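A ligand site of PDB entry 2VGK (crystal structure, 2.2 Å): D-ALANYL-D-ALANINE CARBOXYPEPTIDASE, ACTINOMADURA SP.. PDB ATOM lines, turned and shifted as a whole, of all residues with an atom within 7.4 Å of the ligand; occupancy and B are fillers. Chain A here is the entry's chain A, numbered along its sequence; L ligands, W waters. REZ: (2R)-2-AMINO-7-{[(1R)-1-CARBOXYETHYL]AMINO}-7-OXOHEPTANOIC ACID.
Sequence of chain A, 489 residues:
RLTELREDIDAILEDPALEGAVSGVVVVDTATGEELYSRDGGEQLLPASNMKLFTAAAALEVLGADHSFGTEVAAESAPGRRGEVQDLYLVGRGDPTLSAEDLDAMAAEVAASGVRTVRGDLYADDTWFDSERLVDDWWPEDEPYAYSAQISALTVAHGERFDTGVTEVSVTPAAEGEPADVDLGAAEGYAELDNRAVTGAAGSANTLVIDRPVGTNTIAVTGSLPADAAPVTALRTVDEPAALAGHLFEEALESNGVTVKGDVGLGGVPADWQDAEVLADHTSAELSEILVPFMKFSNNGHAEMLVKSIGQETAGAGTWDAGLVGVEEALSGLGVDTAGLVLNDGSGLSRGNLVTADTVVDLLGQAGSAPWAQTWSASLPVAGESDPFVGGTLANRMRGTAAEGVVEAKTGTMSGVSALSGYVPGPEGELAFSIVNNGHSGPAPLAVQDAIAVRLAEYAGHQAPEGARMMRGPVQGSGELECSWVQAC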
ATOM      1  N   ALA A  48       5.230 -15.821  13.259  1.00  0.00           N
ATOM      2  CA  ALA A  48       5.496 -14.714  14.193  1.00  0.00           C
ATOM      3  C   ALA A  48       6.663 -15.070  15.130  1.00  0.00           C
ATOM      4  O   ALA A  48       7.664 -15.616  14.662  1.00  0.00           O
ATOM      5  CB  ALA A  48       4.226 -14.317  14.962  1.00  0.00           C
ATOM      6  N   SER A  49       6.540 -14.790  16.431  1.00  0.00           N
ATOM      7  CA  SER A  49       7.621 -15.054  17.397  1.00  0.00           C
ATOM      8  C   SER A  49       8.021 -16.519  17.655  1.00  0.00           C
ATOM      9  O   SER A  49       8.999 -16.756  18.349  1.00  0.00           O
ATOM     10  CB  SER A  49       7.350 -14.342  18.730  1.00  0.00           C
ATOM     11  OG  SER A  49       7.289 -12.937  18.573  1.00  0.00           O
ATOM     12  N   LYS A  52      11.598 -17.437  17.110  1.00  0.00           N
ATOM     13  CA  LYS A  52      12.605 -17.231  18.142  1.00  0.00           C
ATOM     14  C   LYS A  52      13.143 -18.544  18.682  1.00  0.00           C
ATOM     15  O   LYS A  52      14.270 -18.591  19.187  1.00  0.00           O
ATOM     16  CB  LYS A  52      12.050 -16.377  19.281  1.00  0.00           C
ATOM     17  CG  LYS A  52      12.255 -14.897  19.052  1.00  0.00           C
ATOM     18  CD  LYS A  52      11.354 -14.041  19.910  1.00  0.00           C
ATOM     19  CE  LYS A  52      11.470 -12.595  19.477  1.00  0.00           C
ATOM     20  NZ  LYS A  52      10.141 -12.011  19.392  1.00  0.00           N
ATOM     21  N   TRP A 139       7.376  -3.036   8.185  1.00  0.00           N
ATOM     22  CA  TRP A 139       6.462  -1.956   7.783  1.00  0.00           C
ATOM     23  C   TRP A 139       6.829  -0.606   8.421  1.00  0.00           C
ATOM     24  O   TRP A 139       6.936  -0.500   9.639  1.00  0.00           O
ATOM     25  CB  TRP A 139       5.041  -2.348   8.167  1.00  0.00           C
ATOM     26  CG  TRP A 139       4.489  -3.542   7.437  1.00  0.00           C
ATOM     27  CD1 TRP A 139       5.183  -4.405   6.628  1.00  0.00           C
ATOM     28  CD2 TRP A 139       3.136  -4.030   7.473  1.00  0.00           C
ATOM     29  NE1 TRP A 139       4.336  -5.396   6.148  1.00  0.00           N
ATOM     30  CE2 TRP A 139       3.079  -5.184   6.651  1.00  0.00           C
ATOM     31  CE3 TRP A 139       1.966  -3.603   8.124  1.00  0.00           C
ATOM     32  CZ2 TRP A 139       1.901  -5.912   6.456  1.00  0.00           C
ATOM     33  CZ3 TRP A 139       0.788  -4.331   7.918  1.00  0.00           C
ATOM     34  CH2 TRP A 139       0.771  -5.466   7.094  1.00  0.00           C
ATOM     35  N   GLU A 141       5.187   2.032   9.167  1.00  0.00           N
ATOM     36  CA  GLU A 141       4.218   2.559  10.134  1.00  0.00           C
ATOM     37  C   GLU A 141       4.307   1.970  11.560  1.00  0.00           C
ATOM     38  O   GLU A 141       3.706   2.508  12.495  1.00  0.00           O
ATOM     39  CB  GLU A 141       2.774   2.504   9.583  1.00  0.00           C
ATOM     40  CG  GLU A 141       2.315   1.144   9.043  1.00  0.00           C
ATOM     41  CD  GLU A 141       2.644   0.913   7.565  1.00  0.00           C
ATOM     42  OE1 GLU A 141       3.019  -0.221   7.209  1.00  0.00           O
ATOM     43  OE2 GLU A 141       2.526   1.861   6.761  1.00  0.00           O
ATOM     44  N   ASP A 142       5.078   0.898  11.713  1.00  0.00           N
ATOM     45  CA  ASP A 142       5.354   0.238  13.001  1.00  0.00           C
ATOM     46  C   ASP A 142       6.604   0.754  13.738  1.00  0.00           C
ATOM     47  O   ASP A 142       6.827   0.428  14.897  1.00  0.00           O
ATOM     48  CB  ASP A 142       5.493  -1.273  12.798  1.00  0.00           C
ATOM     49  CG  ASP A 142       4.179  -1.934  12.405  1.00  0.00           C
ATOM     50  OD1 ASP A 142       3.122  -1.280  12.549  1.00  0.00           O
ATOM     51  OD2 ASP A 142       4.216  -3.097  11.967  1.00  0.00           O
ATOM     52  N   ALA A 146       8.513  -0.244  20.441  1.00  0.00           N
ATOM     53  CA  ALA A 146       9.695  -0.963  20.958  1.00  0.00           C
ATOM     54  C   ALA A 146      10.095  -2.260  20.235  1.00  0.00           C
ATOM     55  O   ALA A 146      11.286  -2.598  20.167  1.00  0.00           O
ATOM     56  CB  ALA A 146       9.538  -1.207  22.472  1.00  0.00           C
ATOM     57  N   TYR A 147       9.119  -2.997  19.701  1.00  0.00           N
ATOM     58  CA  TYR A 147       9.409  -4.231  18.969  1.00  0.00           C
ATOM     59  C   TYR A 147      10.017  -3.981  17.567  1.00  0.00           C
ATOM     60  O   TYR A 147      10.555  -4.903  16.940  1.00  0.00           O
ATOM     61  CB  TYR A 147       8.156  -5.130  18.877  1.00  0.00           C
ATOM     62  CG  TYR A 147       7.042  -4.537  18.021  1.00  0.00           C
ATOM     63  CD1 TYR A 147       7.090  -4.622  16.620  1.00  0.00           C
ATOM     64  CD2 TYR A 147       5.963  -3.891  18.608  1.00  0.00           C
ATOM     65  CE1 TYR A 147       6.091  -4.074  15.833  1.00  0.00           C
ATOM     66  CE2 TYR A 147       4.944  -3.341  17.823  1.00  0.00           C
ATOM     67  CZ  TYR A 147       5.014  -3.438  16.439  1.00  0.00           C
ATOM     68  OH  TYR A 147       4.015  -2.899  15.662  1.00  0.00           O
ATOM     69  N   SER A 148       9.915  -2.729  17.089  1.00  0.00           N
ATOM     70  CA  SER A 148      10.506  -2.320  15.802  1.00  0.00           C
ATOM     71  C   SER A 148      11.708  -1.362  15.980  1.00  0.00           C
ATOM     72  O   SER A 148      12.021  -0.553  15.086  1.00  0.00           O
ATOM     73  CB  SER A 148       9.450  -1.678  14.901  1.00  0.00           C
ATOM     74  OG  SER A 148      10.013  -1.308  13.646  1.00  0.00           O
ATOM     75  N   ASP A 163      14.499  -3.633  27.109  1.00  0.00           N
ATOM     76  CA  ASP A 163      14.015  -3.197  25.794  1.00  0.00           C
ATOM     77  C   ASP A 163      14.999  -2.200  25.178  1.00  0.00           C
ATOM     78  O   ASP A 163      15.179  -1.103  25.697  1.00  0.00           O
ATOM     79  CB  ASP A 163      12.604  -2.585  25.917  1.00  0.00           C
ATOM     80  CG  ASP A 163      11.589  -3.551  26.516  1.00  0.00           C
ATOM     81  OD1 ASP A 163      11.461  -4.700  26.032  1.00  0.00           O
ATOM     82  OD2 ASP A 163      10.908  -3.152  27.486  1.00  0.00           O
ATOM     83  N   PHE A 297       9.542 -12.755  27.579  1.00  0.00           N
ATOM     84  CA  PHE A 297       8.772 -11.568  27.177  1.00  0.00           C
ATOM     85  C   PHE A 297       8.758 -11.340  25.667  1.00  0.00           C
ATOM     86  O   PHE A 297       8.085 -10.425  25.191  1.00  0.00           O
ATOM     87  CB  PHE A 297       9.273 -10.302  27.883  1.00  0.00           C
ATOM     88  CG  PHE A 297       9.259 -10.389  29.378  1.00  0.00           C
ATOM     89  CD1 PHE A 297       8.059 -10.583  30.069  1.00  0.00           C
ATOM     90  CD2 PHE A 297      10.439 -10.291  30.112  1.00  0.00           C
ATOM     91  CE1 PHE A 297       8.045 -10.667  31.453  1.00  0.00           C
ATOM     92  CE2 PHE A 297      10.426 -10.376  31.507  1.00  0.00           C
ATOM     93  CZ  PHE A 297       9.234 -10.569  32.177  1.00  0.00           C
ATOM     94  N   SER A 298       9.510 -12.156  24.944  1.00  0.00           N
ATOM     95  CA  SER A 298       9.545 -12.130  23.476  1.00  0.00           C
ATOM     96  C   SER A 298      10.188 -10.855  22.904  1.00  0.00           C
ATOM     97  O   SER A 298       9.552 -10.076  22.191  1.00  0.00           O
ATOM     98  CB  SER A 298       8.145 -12.366  22.898  1.00  0.00           C
ATOM     99  OG  SER A 298       8.211 -12.863  21.577  1.00  0.00           O
ATOM    100  N   ASN A 299      11.465 -10.672  23.231  1.00  0.00           N
ATOM    101  CA  ASN A 299      12.236  -9.512  22.777  1.00  0.00           C
ATOM    102  C   ASN A 299      12.762  -9.609  21.334  1.00  0.00           C
ATOM    103  O   ASN A 299      13.602 -10.454  21.045  1.00  0.00           O
ATOM    104  CB  ASN A 299      13.397  -9.308  23.736  1.00  0.00           C
ATOM    105  CG  ASN A 299      13.819  -7.869  23.819  1.00  0.00           C
ATOM    106  OD1 ASN A 299      13.743  -7.266  24.882  1.00  0.00           O
ATOM    107  ND2 ASN A 299      14.269  -7.309  22.718  1.00  0.00           N
ATOM    108  N   ASN A 300      12.265  -8.730  20.451  1.00  0.00           N
ATOM    109  CA  ASN A 300      12.666  -8.674  19.033  1.00  0.00           C
ATOM    110  C   ASN A 300      14.106  -8.185  18.829  1.00  0.00           C
ATOM    111  O   ASN A 300      14.870  -8.771  18.069  1.00  0.00           O
ATOM    112  CB  ASN A 300      11.714  -7.766  18.219  1.00  0.00           C
ATOM    113  CG  ASN A 300      10.313  -8.377  17.975  1.00  0.00           C
ATOM    114  OD1 ASN A 300       9.980  -9.469  18.473  1.00  0.00           O
ATOM    115  ND2 ASN A 300       9.499  -7.673  17.195  1.00  0.00           N
ATOM    116  N   SER A 347      13.719 -12.597  14.918  1.00  0.00           N
ATOM    117  CA  SER A 347      12.600 -12.286  15.833  1.00  0.00           C
ATOM    118  C   SER A 347      11.235 -12.825  15.397  1.00  0.00           C
ATOM    119  O   SER A 347      10.377 -13.130  16.237  1.00  0.00           O
ATOM    120  CB  SER A 347      12.492 -10.757  16.034  1.00  0.00           C
ATOM    121  OG  SER A 347      11.965 -10.122  14.877  1.00  0.00           O
ATOM    122  N   GLY A 348      11.030 -12.917  14.087  1.00  0.00           N
ATOM    123  CA  GLY A 348       9.767 -13.376  13.534  1.00  0.00           C
ATOM    124  C   GLY A 348       8.807 -12.255  13.156  1.00  0.00           C
ATOM    125  O   GLY A 348       7.667 -12.531  12.817  1.00  0.00           O
ATOM    126  N   LEU A 349       9.271 -11.007  13.202  1.00  0.00           N
ATOM    127  CA  LEU A 349       8.489  -9.830  12.791  1.00  0.00           C
ATOM    128  C   LEU A 349       8.259  -9.776  11.266  1.00  0.00           C
ATOM    129  O   LEU A 349       7.247  -9.253  10.791  1.00  0.00           O
ATOM    130  CB  LEU A 349       9.202  -8.545  13.268  1.00  0.00           C
ATOM    131  CG  LEU A 349       8.478  -7.223  13.597  1.00  0.00           C
ATOM    132  CD1 LEU A 349       9.478  -6.059  13.706  1.00  0.00           C
ATOM    133  CD2 LEU A 349       7.358  -6.848  12.617  1.00  0.00           C
ATOM    134  N   ARG A 351       7.236 -10.855   7.587  1.00  0.00           N
ATOM    135  CA  ARG A 351       6.243 -11.699   6.892  1.00  0.00           C
ATOM    136  C   ARG A 351       6.889 -12.474   5.737  1.00  0.00           C
ATOM    137  O   ARG A 351       6.204 -13.123   4.939  1.00  0.00           O
ATOM    138  CB  ARG A 351       5.057 -10.851   6.408  1.00  0.00           C
ATOM    139  CG  ARG A 351       4.367 -10.064   7.517  1.00  0.00           C
ATOM    140  CD  ARG A 351       2.995  -9.562   7.082  1.00  0.00           C
ATOM    141  NE  ARG A 351       2.200  -9.053   8.204  1.00  0.00           N
ATOM    142  CZ  ARG A 351       1.201  -9.709   8.788  1.00  0.00           C
ATOM    143  NH1 ARG A 351       0.549  -9.151   9.809  1.00  0.00           N
ATOM    144  NH2 ARG A 351       0.846 -10.933   8.372  1.00  0.00           N
ATOM    145  N   THR A 393       4.768 -14.310  28.749  1.00  0.00           N
ATOM    146  CA  THR A 393       3.568 -14.096  27.922  1.00  0.00           C
ATOM    147  C   THR A 393       2.410 -15.082  28.151  1.00  0.00           C
ATOM    148  O   THR A 393       1.328 -14.945  27.554  1.00  0.00           O
ATOM    149  CB  THR A 393       3.902 -14.057  26.428  1.00  0.00           C
ATOM    150  OG1 THR A 393       4.534 -15.296  26.048  1.00  0.00           O
ATOM    151  CG2 THR A 393       4.815 -12.873  26.103  1.00  0.00           C
ATOM    152  N   LYS A 410       6.440 -21.374  23.795  1.00  0.00           N
ATOM    153  CA  LYS A 410       6.608 -20.057  23.175  1.00  0.00           C
ATOM    154  C   LYS A 410       5.328 -19.652  22.429  1.00  0.00           C
ATOM    155  O   LYS A 410       4.663 -20.484  21.807  1.00  0.00           O
ATOM    156  CB  LYS A 410       7.822 -20.039  22.228  1.00  0.00           C
ATOM    157  CG  LYS A 410       8.239 -18.659  21.699  1.00  0.00           C
ATOM    158  CD  LYS A 410       8.846 -17.763  22.789  1.00  0.00           C
ATOM    159  CE  LYS A 410       9.050 -16.309  22.329  1.00  0.00           C
ATOM    160  NZ  LYS A 410       7.787 -15.563  22.041  1.00  0.00           N
ATOM    161  N   GLY A 412       3.399 -16.337  19.890  1.00  0.00           N
ATOM    162  CA  GLY A 412       3.744 -15.475  18.774  1.00  0.00           C
ATOM    163  C   GLY A 412       2.496 -15.071  18.046  1.00  0.00           C
ATOM    164  O   GLY A 412       1.896 -15.894  17.357  1.00  0.00           O
ATOM    165  N   THR A 413       2.107 -13.804  18.205  1.00  0.00           N
ATOM    166  CA  THR A 413       0.891 -13.252  17.577  1.00  0.00           C
ATOM    167  C   THR A 413       1.125 -11.943  16.800  1.00  0.00           C
ATOM    168  O   THR A 413       1.800 -11.018  17.283  1.00  0.00           O
ATOM    169  CB  THR A 413      -0.249 -13.053  18.622  1.00  0.00           C
ATOM    170  OG1 THR A 413      -0.755 -14.339  19.041  1.00  0.00           O
ATOM    171  CG2 THR A 413      -1.404 -12.235  18.055  1.00  0.00           C
ATOM    172  N   MET A 414       0.523 -11.887  15.618  1.00  0.00           N
ATOM    173  CA  MET A 414       0.552 -10.751  14.715  1.00  0.00           C
ATOM    174  C   MET A 414      -0.846 -10.645  14.074  1.00  0.00           C
ATOM    175  O   MET A 414      -1.647 -11.569  14.224  1.00  0.00           O
ATOM    176  CB  MET A 414       1.597 -11.047  13.636  1.00  0.00           C
ATOM    177  CG  MET A 414       2.233  -9.851  13.014  1.00  0.00           C
ATOM    178  SD  MET A 414       3.906 -10.212  12.482  1.00  0.00           S
ATOM    179  CE  MET A 414       3.597 -11.432  11.189  1.00  0.00           C
ATOM    180  N   SER A 415      -1.135  -9.575  13.347  1.00  0.00           N
ATOM    181  CA  SER A 415      -2.342  -9.540  12.497  1.00  0.00           C
ATOM    182  C   SER A 415      -2.341 -10.723  11.530  1.00  0.00           C
ATOM    183  O   SER A 415      -1.398 -10.892  10.753  1.00  0.00           O
ATOM    184  CB  SER A 415      -2.431  -8.252  11.698  1.00  0.00           C
ATOM    185  OG  SER A 415      -2.788  -7.158  12.513  1.00  0.00           O
ATOM    186  N   GLY A 416      -3.389 -11.559  11.593  1.00  0.00           N
ATOM    187  CA  GLY A 416      -3.554 -12.699  10.680  1.00  0.00           C
ATOM    188  C   GLY A 416      -2.775 -13.984  10.969  1.00  0.00           C
ATOM    189  O   GLY A 416      -2.959 -14.987  10.272  1.00  0.00           O
HETATM  190  CA1 REZ L   1       3.703  -7.407  16.963  1.00  0.00           C
HETATM  191  CB1 REZ L   1       3.826  -7.323  15.449  1.00  0.00           C
HETATM  192  CG1 REZ L   1       2.776  -6.377  14.895  1.00  0.00           C
HETATM  193  CD1 REZ L   1       2.994  -6.145  13.405  1.00  0.00           C
HETATM  194  CE1 REZ L   1       1.852  -5.365  12.756  1.00  0.00           C
HETATM  195  NZ1 REZ L   1       2.331  -4.784  11.512  1.00  0.00           N
HETATM  196  CZ1 REZ L   1       0.682  -6.271  12.466  1.00  0.00           C
HETATM  197  OH1 REZ L   1       0.686  -6.892  11.389  1.00  0.00           O
HETATM  198  OH2 REZ L   1      -0.221  -6.365  13.314  1.00  0.00           O
HETATM  199  C1  REZ L   1       4.890  -8.069  17.641  1.00  0.00           C
HETATM  200  O1  REZ L   1       5.556  -8.935  17.085  1.00  0.00           O
HETATM  201  N   REZ L   1       5.078  -7.626  18.889  1.00  0.00           N
HETATM  202  CA  REZ L   1       6.115  -8.019  19.846  1.00  0.00           C
HETATM  203  CB  REZ L   1       6.121  -9.534  20.086  1.00  0.00           C
HETATM  204  C   REZ L   1       5.923  -7.308  21.162  1.00  0.00           C
HETATM  205  O   REZ L   1       4.747  -7.096  21.558  1.00  0.00           O
HETATM  206  OXT REZ L   1       6.931  -6.924  21.807  1.00  0.00           O
HETATM  207  O   HOH W   1       1.350  -8.854  18.821  1.00  0.00           O
HETATM  208  O   HOH W   2       3.647  -6.535   9.768  1.00  0.00           O
HETATM  209  O   HOH W   3       8.391  -7.328  23.952  1.00  0.00           O
HETATM  210  O   HOH W   4       2.679  -5.719  20.136  1.00  0.00           O
HETATM  211  O   HOH W   5       5.190 -12.041  17.274  1.00  0.00           O
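The guanidinium group of Arg 351 is in salt-bridge range of an oxygen (OH1) of the ligand (2.8 Å). OH2 of the ligand lies within hydrogen-bond range of OG of Ser 415, 2.8 Å away. The backbone NH (N) of Ser 415 sits close to an oxygen (OH2) of the ligand, at 3.3 Å. The side-chain carboxylate (OD2) of Asp 142 is in salt-bridge range of a nitrogen (NZ1) of the ligand, at 2.6 Å.
The side-chain hydroxyl of Ser 49 sits at hydrogen-bond distance from the side-chain hydroxyl of Ser 298 (3.1 Å). The side-chain amino group (NZ) of Lys 52 sits at hydrogen-bond distance from the side-chain hydroxyl (OG) of Ser 49 (3.1 Å). The guanidinium group (NH1) of Arg 351 lies within hydrogen-bond range of the backbone carbonyl oxygen (O) of Ser 415, 2.8 Å away. O of Tyr 147 is in hydrogen-bond range of ND2 of Asn 300 (3.0 Å).
OG of Ser 49 touches CB of the ligand (3.9 Å). CE3 of Trp 139 touches NZ1 of the ligand, at 3.6 Å. Tyr 147 touches the ligand. Met 414 touches the ligand. Hydrophobic or aromatic side chains within 4 Å of the ligand: Trp 139, Tyr 147 and Met 414. Within 4 Å of the ligand: Ser 49, Trp 139, Asp 142, Tyr 147, Arg 351, Met 414 and Ser 415.
Water W3 lies within hydrogen-bond range of an oxygen (OXT) of the ligand, the backbone carbonyl oxygen (O) of Phe 297 and the backbone carbonyl oxygen (O) of Ser 298. Water W2 bridges a nitrogen (NZ1) of the ligand and the guanidinium group (NE) of Arg 351. Water W5 bridges OG of Ser 49 (2.6 Å) and O1 of the ligand (3.1 Å).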
